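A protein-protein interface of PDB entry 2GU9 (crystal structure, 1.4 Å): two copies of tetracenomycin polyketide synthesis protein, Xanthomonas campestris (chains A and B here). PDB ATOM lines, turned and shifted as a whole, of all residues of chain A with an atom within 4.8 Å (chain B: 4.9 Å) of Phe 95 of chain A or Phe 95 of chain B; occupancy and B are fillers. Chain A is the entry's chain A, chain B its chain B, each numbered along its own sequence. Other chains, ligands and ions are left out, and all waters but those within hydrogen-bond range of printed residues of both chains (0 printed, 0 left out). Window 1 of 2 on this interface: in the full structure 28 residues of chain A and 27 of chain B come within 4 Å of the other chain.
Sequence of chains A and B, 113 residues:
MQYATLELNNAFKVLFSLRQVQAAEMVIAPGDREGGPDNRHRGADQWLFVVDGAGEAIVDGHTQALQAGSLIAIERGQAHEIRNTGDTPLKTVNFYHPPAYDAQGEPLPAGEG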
ATOM      1  N   VAL A  21      -7.291  18.225  26.512  1.00  0.00           N
ATOM      2  CA  VAL A  21      -5.995  18.795  26.149  1.00  0.00           C
ATOM      3  C   VAL A  21      -5.465  17.925  25.007  1.00  0.00           C
ATOM      4  O   VAL A  21      -5.489  16.693  25.088  1.00  0.00           O
ATOM      5  CB  VAL A  21      -4.989  18.798  27.319  1.00  0.00           C
ATOM      6  CG1 VAL A  21      -3.633  19.269  26.826  1.00  0.00           C
ATOM      7  CG2 VAL A  21      -5.475  19.731  28.422  1.00  0.00           C
ATOM      8  N   GLN A  22      -5.003  18.575  23.944  1.00  0.00           N
ATOM      9  CA  GLN A  22      -4.510  17.877  22.759  1.00  0.00           C
ATOM     10  C   GLN A  22      -3.088  18.288  22.414  1.00  0.00           C
ATOM     11  O   GLN A  22      -2.766  19.474  22.388  1.00  0.00           O
ATOM     12  CB  GLN A  22      -5.446  18.187  21.588  1.00  0.00           C
ATOM     13  CG  GLN A  22      -4.963  17.750  20.217  1.00  0.00           C
ATOM     14  CD  GLN A  22      -6.006  18.011  19.146  1.00  0.00           C
ATOM     15  OE1 GLN A  22      -6.605  17.082  18.599  1.00  0.00           O
ATOM     16  NE2 GLN A  22      -6.241  19.281  18.853  1.00  0.00           N
ATOM     17  N   ALA A  23      -2.241  17.304  22.140  1.00  0.00           N
ATOM     18  CA  ALA A  23      -0.851  17.575  21.798  1.00  0.00           C
ATOM     19  C   ALA A  23      -0.600  17.418  20.301  1.00  0.00           C
ATOM     20  O   ALA A  23      -1.217  16.589  19.635  1.00  0.00           O
ATOM     21  CB  ALA A  23       0.066  16.646  22.590  1.00  0.00           C
ATOM     22  N   ASP A  45      -6.954  27.496  23.476  1.00  0.00           N
ATOM     23  CA  ASP A  45      -5.720  28.108  23.941  1.00  0.00           C
ATOM     24  C   ASP A  45      -4.612  27.298  23.277  1.00  0.00           C
ATOM     25  O   ASP A  45      -4.766  26.093  23.058  1.00  0.00           O
ATOM     26  CB  ASP A  45      -5.573  27.954  25.458  1.00  0.00           C
ATOM     27  CG  ASP A  45      -6.745  28.524  26.233  1.00  0.00           C
ATOM     28  OD1 ASP A  45      -7.018  27.990  27.324  1.00  0.00           O
ATOM     29  OD2 ASP A  45      -7.369  29.500  25.770  1.00  0.00           O
ATOM     30  N   GLN A  46      -3.507  27.947  22.939  1.00  0.00           N
ATOM     31  CA  GLN A  46      -2.385  27.231  22.346  1.00  0.00           C
ATOM     32  C   GLN A  46      -1.128  27.453  23.173  1.00  0.00           C
ATOM     33  O   GLN A  46      -0.711  28.593  23.404  1.00  0.00           O
ATOM     34  CB  GLN A  46      -2.126  27.674  20.900  1.00  0.00           C
ATOM     35  CG  GLN A  46      -0.862  27.030  20.300  1.00  0.00           C
ATOM     36  CD  GLN A  46      -0.634  27.363  18.831  1.00  0.00           C
ATOM     37  OE1 GLN A  46      -1.274  28.243  18.271  1.00  0.00           O
ATOM     38  NE2 GLN A  46       0.302  26.660  18.210  1.00  0.00           N
ATOM     39  N   TRP A  47      -0.547  26.356  23.646  1.00  0.00           N
ATOM     40  CA  TRP A  47       0.691  26.390  24.412  1.00  0.00           C
ATOM     41  C   TRP A  47       1.750  25.872  23.446  1.00  0.00           C
ATOM     42  O   TRP A  47       1.616  24.779  22.897  1.00  0.00           O
ATOM     43  CB  TRP A  47       0.629  25.462  25.628  1.00  0.00           C
ATOM     44  CG  TRP A  47      -0.353  25.851  26.687  1.00  0.00           C
ATOM     45  CD1 TRP A  47      -1.713  25.732  26.639  1.00  0.00           C
ATOM     46  CD2 TRP A  47      -0.040  26.391  27.975  1.00  0.00           C
ATOM     47  NE1 TRP A  47      -2.267  26.159  27.827  1.00  0.00           N
ATOM     48  CE2 TRP A  47      -1.261  26.570  28.662  1.00  0.00           C
ATOM     49  CE3 TRP A  47       1.158  26.738  28.617  1.00  0.00           C
ATOM     50  CZ2 TRP A  47      -1.322  27.083  29.963  1.00  0.00           C
ATOM     51  CZ3 TRP A  47       1.097  27.246  29.913  1.00  0.00           C
ATOM     52  CH2 TRP A  47      -0.135  27.414  30.570  1.00  0.00           C
ATOM     53  N   LEU A  71       8.545  29.154  25.848  1.00  0.00           N
ATOM     54  CA  LEU A  71       7.228  28.606  26.122  1.00  0.00           C
ATOM     55  C   LEU A  71       6.262  29.769  26.067  1.00  0.00           C
ATOM     56  O   LEU A  71       6.435  30.773  26.769  1.00  0.00           O
ATOM     57  CB  LEU A  71       7.145  27.963  27.504  1.00  0.00           C
ATOM     58  CG  LEU A  71       5.717  27.508  27.856  1.00  0.00           C
ATOM     59  CD1 LEU A  71       5.290  26.370  26.922  1.00  0.00           C
ATOM     60  CD2 LEU A  71       5.653  27.058  29.311  1.00  0.00           C
ATOM     61  N   VAL A  93       6.492  21.702  20.023  1.00  0.00           N
ATOM     62  CA  VAL A  93       5.489  20.774  20.524  1.00  0.00           C
ATOM     63  C   VAL A  93       4.386  21.695  21.033  1.00  0.00           C
ATOM     64  O   VAL A  93       4.658  22.707  21.686  1.00  0.00           O
ATOM     65  CB  VAL A  93       6.040  19.847  21.641  1.00  0.00           C
ATOM     66  CG1 VAL A  93       6.534  20.654  22.817  1.00  0.00           C
ATOM     67  CG2 VAL A  93       4.957  18.860  22.069  1.00  0.00           C
ATOM     68  N   ASN A  94       3.142  21.357  20.709  1.00  0.00           N
ATOM     69  CA  ASN A  94       2.006  22.199  21.061  1.00  0.00           C
ATOM     70  C   ASN A  94       0.898  21.510  21.828  1.00  0.00           C
ATOM     71  O   ASN A  94       0.632  20.330  21.628  1.00  0.00           O
ATOM     72  CB  ASN A  94       1.402  22.789  19.789  1.00  0.00           C
ATOM     73  CG  ASN A  94       2.385  23.627  19.014  1.00  0.00           C
ATOM     74  OD1 ASN A  94       2.350  24.852  19.082  1.00  0.00           O
ATOM     75  ND2 ASN A  94       3.281  22.971  18.280  1.00  0.00           N
ATOM     76  N   PHE A  95       0.242  22.272  22.696  1.00  0.00           N
ATOM     77  CA  PHE A  95      -0.873  21.757  23.470  1.00  0.00           C
ATOM     78  C   PHE A  95      -2.060  22.691  23.309  1.00  0.00           C
ATOM     79  O   PHE A  95      -1.943  23.908  23.472  1.00  0.00           O
ATOM     80  CB  PHE A  95      -0.493  21.617  24.945  1.00  0.00           C
ATOM     81  CG  PHE A  95       0.718  20.760  25.168  1.00  0.00           C
ATOM     82  CD1 PHE A  95       1.995  21.292  25.007  1.00  0.00           C
ATOM     83  CD2 PHE A  95       0.589  19.407  25.481  1.00  0.00           C
ATOM     84  CE1 PHE A  95       3.127  20.494  25.149  1.00  0.00           C
ATOM     85  CE2 PHE A  95       1.721  18.594  25.624  1.00  0.00           C
ATOM     86  CZ  PHE A  95       2.991  19.141  25.458  1.00  0.00           C
ATOM     87  N   TYR A  96      -3.204  22.111  22.972  1.00  0.00           N
ATOM     88  CA  TYR A  96      -4.414  22.887  22.772  1.00  0.00           C
ATOM     89  C   TYR A  96      -5.476  22.545  23.801  1.00  0.00           C
ATOM     90  O   TYR A  96      -5.728  21.374  24.101  1.00  0.00           O
ATOM     91  CB  TYR A  96      -4.964  22.655  21.360  1.00  0.00           C
ATOM     92  CG  TYR A  96      -3.961  22.956  20.269  1.00  0.00           C
ATOM     93  CD1 TYR A  96      -3.104  21.965  19.791  1.00  0.00           C
ATOM     94  CD2 TYR A  96      -3.857  24.237  19.724  1.00  0.00           C
ATOM     95  CE1 TYR A  96      -2.169  22.240  18.800  1.00  0.00           C
ATOM     96  CE2 TYR A  96      -2.922  24.526  18.730  1.00  0.00           C
ATOM     97  CZ  TYR A  96      -2.084  23.520  18.275  1.00  0.00           C
ATOM     98  OH  TYR A  96      -1.164  23.790  17.287  1.00  0.00           O
ATOM     99  N   HIS A  97      -6.091  23.585  24.347  1.00  0.00           N
ATOM    100  CA  HIS A  97      -7.137  23.416  25.341  1.00  0.00           C
ATOM    101  C   HIS A  97      -8.282  24.370  25.040  1.00  0.00           C
ATOM    102  O   HIS A  97      -8.119  25.587  25.133  1.00  0.00           O
ATOM    103  CB  HIS A  97      -6.594  23.699  26.744  1.00  0.00           C
ATOM    104  CG  HIS A  97      -7.615  23.537  27.824  1.00  0.00           C
ATOM    105  ND1 HIS A  97      -7.776  24.452  28.840  1.00  0.00           N
ATOM    106  CD2 HIS A  97      -8.542  22.572  28.037  1.00  0.00           C
ATOM    107  CE1 HIS A  97      -8.760  24.061  29.632  1.00  0.00           C
ATOM    108  NE2 HIS A  97      -9.243  22.923  29.166  1.00  0.00           N
ATOM    109  N   VAL B  21      -4.709  25.165  32.952  1.00  0.00           N
ATOM    110  CA  VAL B  21      -3.554  24.389  32.516  1.00  0.00           C
ATOM    111  C   VAL B  21      -2.350  25.127  33.089  1.00  0.00           C
ATOM    112  O   VAL B  21      -2.236  26.351  32.965  1.00  0.00           O
ATOM    113  CB  VAL B  21      -3.445  24.285  30.982  1.00  0.00           C
ATOM    114  CG1 VAL B  21      -2.132  23.597  30.599  1.00  0.00           C
ATOM    115  CG2 VAL B  21      -4.612  23.471  30.442  1.00  0.00           C
ATOM    116  N   GLN B  22      -1.465  24.373  33.730  1.00  0.00           N
ATOM    117  CA  GLN B  22      -0.288  24.943  34.376  1.00  0.00           C
ATOM    118  C   GLN B  22       1.005  24.329  33.861  1.00  0.00           C
ATOM    119  O   GLN B  22       1.118  23.114  33.737  1.00  0.00           O
ATOM    120  CB  GLN B  22      -0.409  24.732  35.887  1.00  0.00           C
ATOM    121  CG  GLN B  22       0.833  25.052  36.701  1.00  0.00           C
ATOM    122  CD  GLN B  22       0.604  24.811  38.179  1.00  0.00           C
ATOM    123  OE1 GLN B  22       0.350  23.682  38.603  1.00  0.00           O
ATOM    124  NE2 GLN B  22       0.679  25.874  38.970  1.00  0.00           N
ATOM    125  N   ALA B  23       1.978  25.178  33.559  1.00  0.00           N
ATOM    126  CA  ALA B  23       3.262  24.706  33.062  1.00  0.00           C
ATOM    127  C   ALA B  23       4.337  24.771  34.143  1.00  0.00           C
ATOM    128  O   ALA B  23       4.318  25.645  35.011  1.00  0.00           O
ATOM    129  CB  ALA B  23       3.691  25.532  31.853  1.00  0.00           C
ATOM    130  N   ASP B  45      -3.939  15.821  35.611  1.00  0.00           N
ATOM    131  CA  ASP B  45      -3.275  15.051  34.570  1.00  0.00           C
ATOM    132  C   ASP B  45      -1.903  15.689  34.443  1.00  0.00           C
ATOM    133  O   ASP B  45      -1.755  16.895  34.664  1.00  0.00           O
ATOM    134  CB  ASP B  45      -3.980  15.179  33.216  1.00  0.00           C
ATOM    135  CG  ASP B  45      -5.457  14.855  33.282  1.00  0.00           C
ATOM    136  OD1 ASP B  45      -5.834  13.919  34.010  1.00  0.00           O
ATOM    137  OD2 ASP B  45      -6.231  15.537  32.584  1.00  0.00           O
ATOM    138  N   GLN B  46      -0.899  14.893  34.103  1.00  0.00           N
ATOM    139  CA  GLN B  46       0.446  15.419  33.918  1.00  0.00           C
ATOM    140  C   GLN B  46       0.941  15.086  32.517  1.00  0.00           C
ATOM    141  O   GLN B  46       0.991  13.920  32.125  1.00  0.00           O
ATOM    142  CB  GLN B  46       1.430  14.844  34.947  1.00  0.00           C
ATOM    143  CG  GLN B  46       2.863  15.381  34.757  1.00  0.00           C
ATOM    144  CD  GLN B  46       3.875  14.860  35.770  1.00  0.00           C
ATOM    145  OE1 GLN B  46       5.065  15.235  35.660  1.00  0.00           O
ATOM    146  NE2 GLN B  46       3.497  14.084  36.667  1.00  0.00           N
ATOM    147  N   TRP B  47       1.286  16.119  31.760  1.00  0.00           N
ATOM    148  CA  TRP B  47       1.825  15.955  30.417  1.00  0.00           C
ATOM    149  C   TRP B  47       3.299  16.284  30.576  1.00  0.00           C
ATOM    150  O   TRP B  47       3.643  17.362  31.053  1.00  0.00           O
ATOM    151  CB  TRP B  47       1.188  16.940  29.436  1.00  0.00           C
ATOM    152  CG  TRP B  47      -0.262  16.703  29.158  1.00  0.00           C
ATOM    153  CD1 TRP B  47      -1.318  16.967  29.983  1.00  0.00           C
ATOM    154  CD2 TRP B  47      -0.817  16.184  27.946  1.00  0.00           C
ATOM    155  NE1 TRP B  47      -2.502  16.651  29.352  1.00  0.00           N
ATOM    156  CE2 TRP B  47      -2.222  16.169  28.100  1.00  0.00           C
ATOM    157  CE3 TRP B  47      -0.263  15.733  26.738  1.00  0.00           C
ATOM    158  CZ2 TRP B  47      -3.082  15.720  27.092  1.00  0.00           C
ATOM    159  CZ3 TRP B  47      -1.118  15.286  25.735  1.00  0.00           C
ATOM    160  CH2 TRP B  47      -2.514  15.285  25.919  1.00  0.00           C
ATOM    161  N   LEU B  71       6.915  12.174  24.803  1.00  0.00           N
ATOM    162  CA  LEU B  71       5.779  12.920  25.313  1.00  0.00           C
ATOM    163  C   LEU B  71       4.888  11.888  25.975  1.00  0.00           C
ATOM    164  O   LEU B  71       4.513  10.889  25.358  1.00  0.00           O
ATOM    165  CB  LEU B  71       5.008  13.618  24.196  1.00  0.00           C
ATOM    166  CG  LEU B  71       3.731  14.302  24.703  1.00  0.00           C
ATOM    167  CD1 LEU B  71       4.119  15.445  25.641  1.00  0.00           C
ATOM    168  CD2 LEU B  71       2.904  14.832  23.539  1.00  0.00           C
ATOM    169  N   VAL B  93       9.652  19.555  30.496  1.00  0.00           N
ATOM    170  CA  VAL B  93       8.681  20.633  30.585  1.00  0.00           C
ATOM    171  C   VAL B  93       7.369  19.899  30.822  1.00  0.00           C
ATOM    172  O   VAL B  93       7.053  18.920  30.136  1.00  0.00           O
ATOM    173  CB  VAL B  93       8.644  21.518  29.301  1.00  0.00           C
ATOM    174  CG1 VAL B  93       8.278  20.698  28.084  1.00  0.00           C
ATOM    175  CG2 VAL B  93       7.655  22.668  29.493  1.00  0.00           C
ATOM    176  N   ASN B  94       6.625  20.356  31.820  1.00  0.00           N
ATOM    177  CA  ASN B  94       5.378  19.704  32.202  1.00  0.00           C
ATOM    178  C   ASN B  94       4.153  20.602  32.177  1.00  0.00           C
ATOM    179  O   ASN B  94       4.246  21.807  32.412  1.00  0.00           O
ATOM    180  CB  ASN B  94       5.519  19.130  33.609  1.00  0.00           C
ATOM    181  CG  ASN B  94       6.650  18.144  33.724  1.00  0.00           C
ATOM    182  OD1 ASN B  94       6.430  16.937  33.746  1.00  0.00           O
ATOM    183  ND2 ASN B  94       7.879  18.656  33.785  1.00  0.00           N
ATOM    184  N   PHE B  95       3.004  19.993  31.899  1.00  0.00           N
ATOM    185  CA  PHE B  95       1.734  20.706  31.883  1.00  0.00           C
ATOM    186  C   PHE B  95       0.734  19.925  32.715  1.00  0.00           C
ATOM    187  O   PHE B  95       0.517  18.729  32.500  1.00  0.00           O
ATOM    188  CB  PHE B  95       1.216  20.876  30.456  1.00  0.00           C
ATOM    189  CG  PHE B  95       2.194  21.538  29.539  1.00  0.00           C
ATOM    190  CD1 PHE B  95       3.216  20.801  28.947  1.00  0.00           C
ATOM    191  CD2 PHE B  95       2.130  22.909  29.299  1.00  0.00           C
ATOM    192  CE1 PHE B  95       4.160  21.416  28.136  1.00  0.00           C
ATOM    193  CE2 PHE B  95       3.072  23.535  28.488  1.00  0.00           C
ATOM    194  CZ  PHE B  95       4.089  22.789  27.905  1.00  0.00           C
ATOM    195  N   TYR B  96       0.125  20.614  33.670  1.00  0.00           N
ATOM    196  CA  TYR B  96      -0.848  20.003  34.569  1.00  0.00           C
ATOM    197  C   TYR B  96      -2.251  20.531  34.311  1.00  0.00           C
ATOM    198  O   TYR B  96      -2.457  21.738  34.152  1.00  0.00           O
ATOM    199  CB  TYR B  96      -0.445  20.284  36.015  1.00  0.00           C
ATOM    200  CG  TYR B  96       0.943  19.787  36.332  1.00  0.00           C
ATOM    201  CD1 TYR B  96       1.159  18.464  36.710  1.00  0.00           C
ATOM    202  CD2 TYR B  96       2.049  20.630  36.218  1.00  0.00           C
ATOM    203  CE1 TYR B  96       2.439  17.990  36.972  1.00  0.00           C
ATOM    204  CE2 TYR B  96       3.332  20.164  36.469  1.00  0.00           C
ATOM    205  CZ  TYR B  96       3.520  18.845  36.848  1.00  0.00           C
ATOM    206  OH  TYR B  96       4.786  18.385  37.110  1.00  0.00           O
ATOM    207  N   HIS B  97      -3.211  19.613  34.258  1.00  0.00           N
ATOM    208  CA  HIS B  97      -4.608  19.964  34.025  1.00  0.00           C
ATOM    209  C   HIS B  97      -5.489  19.185  34.993  1.00  0.00           C
ATOM    210  O   HIS B  97      -5.572  17.963  34.905  1.00  0.00           O
ATOM    211  CB  HIS B  97      -5.024  19.619  32.591  1.00  0.00           C
ATOM    212  CG  HIS B  97      -6.442  19.981  32.277  1.00  0.00           C
ATOM    213  ND1 HIS B  97      -7.281  19.163  31.549  1.00  0.00           N
ATOM    214  CD2 HIS B  97      -7.170  21.078  32.591  1.00  0.00           C
ATOM    215  CE1 HIS B  97      -8.465  19.741  31.430  1.00  0.00           C
ATOM    216  NE2 HIS B  97      -8.424  20.904  32.054  1.00  0.00           N
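O of His 97 of chain A lies within hydrogen-bond range of N of Asp 45 of chain A (2.8 Å). The backbone carbonyl oxygen (O) of Phe 95 of chain A lies within hydrogen-bond range of the backbone NH (N) of Trp 47 of chain A. The backbone carbonyl oxygen (O) of His 97 of chain B lies within hydrogen-bond range of the backbone NH (N) of Asp 45 of chain B, 2.8 Å away. The backbone carbonyl oxygen (O) of Phe 95 of chain B is in hydrogen-bond range of the backbone NH (N) of Trp 47 of chain B.
Val 21 of chain A touches Trp 47 of chain B (O to CZ2, 3.3 Å). Trp 47 of chain B touches Ala 23 of chain A (CZ3 to CB, 3.6 Å). Trp 47 of chain A touches Ala 23 of chain B. Phe 95 of chain B touches Trp 47 of chain A. Leu 71 of chain A touches Ala 23 of chain B (CD2 to CB, 3.6 Å). Leu 71 of chain A touches Phe 95 of chain B (CD1 to CZ, 3.9 Å). Phe 95 of chain A touches Trp 47 of chain B (CE2 to CE3, 3.7 Å). CD1 of Leu 71 of chain B touches CZ of Phe 95 of chain A, 3.9 Å away. Phe 95 of chain B touches Phe 95 of chain A (CE1 to CE1, 3.3 Å). His 97 of chain A touches Val 21 of chain B (ND1 to CG2, 3.7 Å).
Of the printed residues of chain B, Trp 47 of chain A touches Val 21 (3.2 Å), Ala 23 (3.7 Å) and Phe 95 (3.7 Å). Val 93 of chain A touches none of the printed residues of chain B. Printed residues of chain B within 4 Å of Phe 95 of chain A: Trp 47, Leu 71 and Phe 95. Of the printed residues of chain B, His 97 of chain A touches Val 21 (3.7 Å) and His 97 (3.6 Å). Of the printed residues of chain A, Ala 23 of chain B touches Trp 47 (3.7 Å) and Leu 71 (3.6 Å). Asp 45 of chain B touches none of the printed residues of chain A. Of the printed residues of chain A, Trp 47 of chain B touches Val 21, Ala 23 and Phe 95. Printed residues of chain A within 4 Å of Leu 71 of chain B: Ala 23 (3.5 Å) and Phe 95 (3.9 Å). Phe 95 of chain B touches just these residues of chain A: Trp 47 (3.7 Å), Leu 71 (3.9 Å) and Phe 95 (3.3 Å). The nearest printed residue of chain B that does not touch Phe 95 of chain A is Val 93 of chain B (5.9 Å). The nearest printed residue of chain A that does not touch Phe 95 of chain B is Val 93 of chain A (5.9 Å). The nearest printed residue of chain B that does not touch His 97 of chain A is Gln 22 of chain B (8.0 Å).
Printed residues of chain A that touch a printed residue of chain B: Val 21, Ala 23, Trp 47, Leu 71, Phe 95 and His 97. Hydrophobic or aromatic side chains of chain A that line the printed part of chain B: Val 21, Ala 23, Trp 47, Leu 71, Phe 95 and His 97. Of the 12 printed residues of chain B, 6 touch a printed residue of chain A. Printed residues of chain B that touch a printed residue of chain A: Val 21, Ala 23, Trp 47, Leu 71, Phe 95 and His 97. Hydrophobic or aromatic side chains of chain B within 4 Å of the printed part of chain A: Val 21, Ala 23, Trp 47, Leu 71, Phe 95 and His 97.
Val 21 of chain A touches Trp 47 of chain B, and with the chains exchanged Trp 47 of chain A touches Val 21 of chain B. Val 21 of chain A touches His 97 of chain B, and with the chains exchanged His 97 of chain A touches Val 21 of chain B. Trp 47 of chain A touches Phe 95 of chain B, and with the chains exchanged Phe 95 of chain A touches Trp 47 of chain B. Leu 71 of chain A touches Phe 95 of chain B, and with the chains exchanged Phe 95 of chain A touches Leu 71 of chain B. Positions printed for both chains: 21, 22, 23, 45, 46, 47, 71, 93, 94, 95, 96 and 97. Of the 14 pairs that touch across the chains among the printed residues, 14 have their exchanged pair printed and touching as well.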
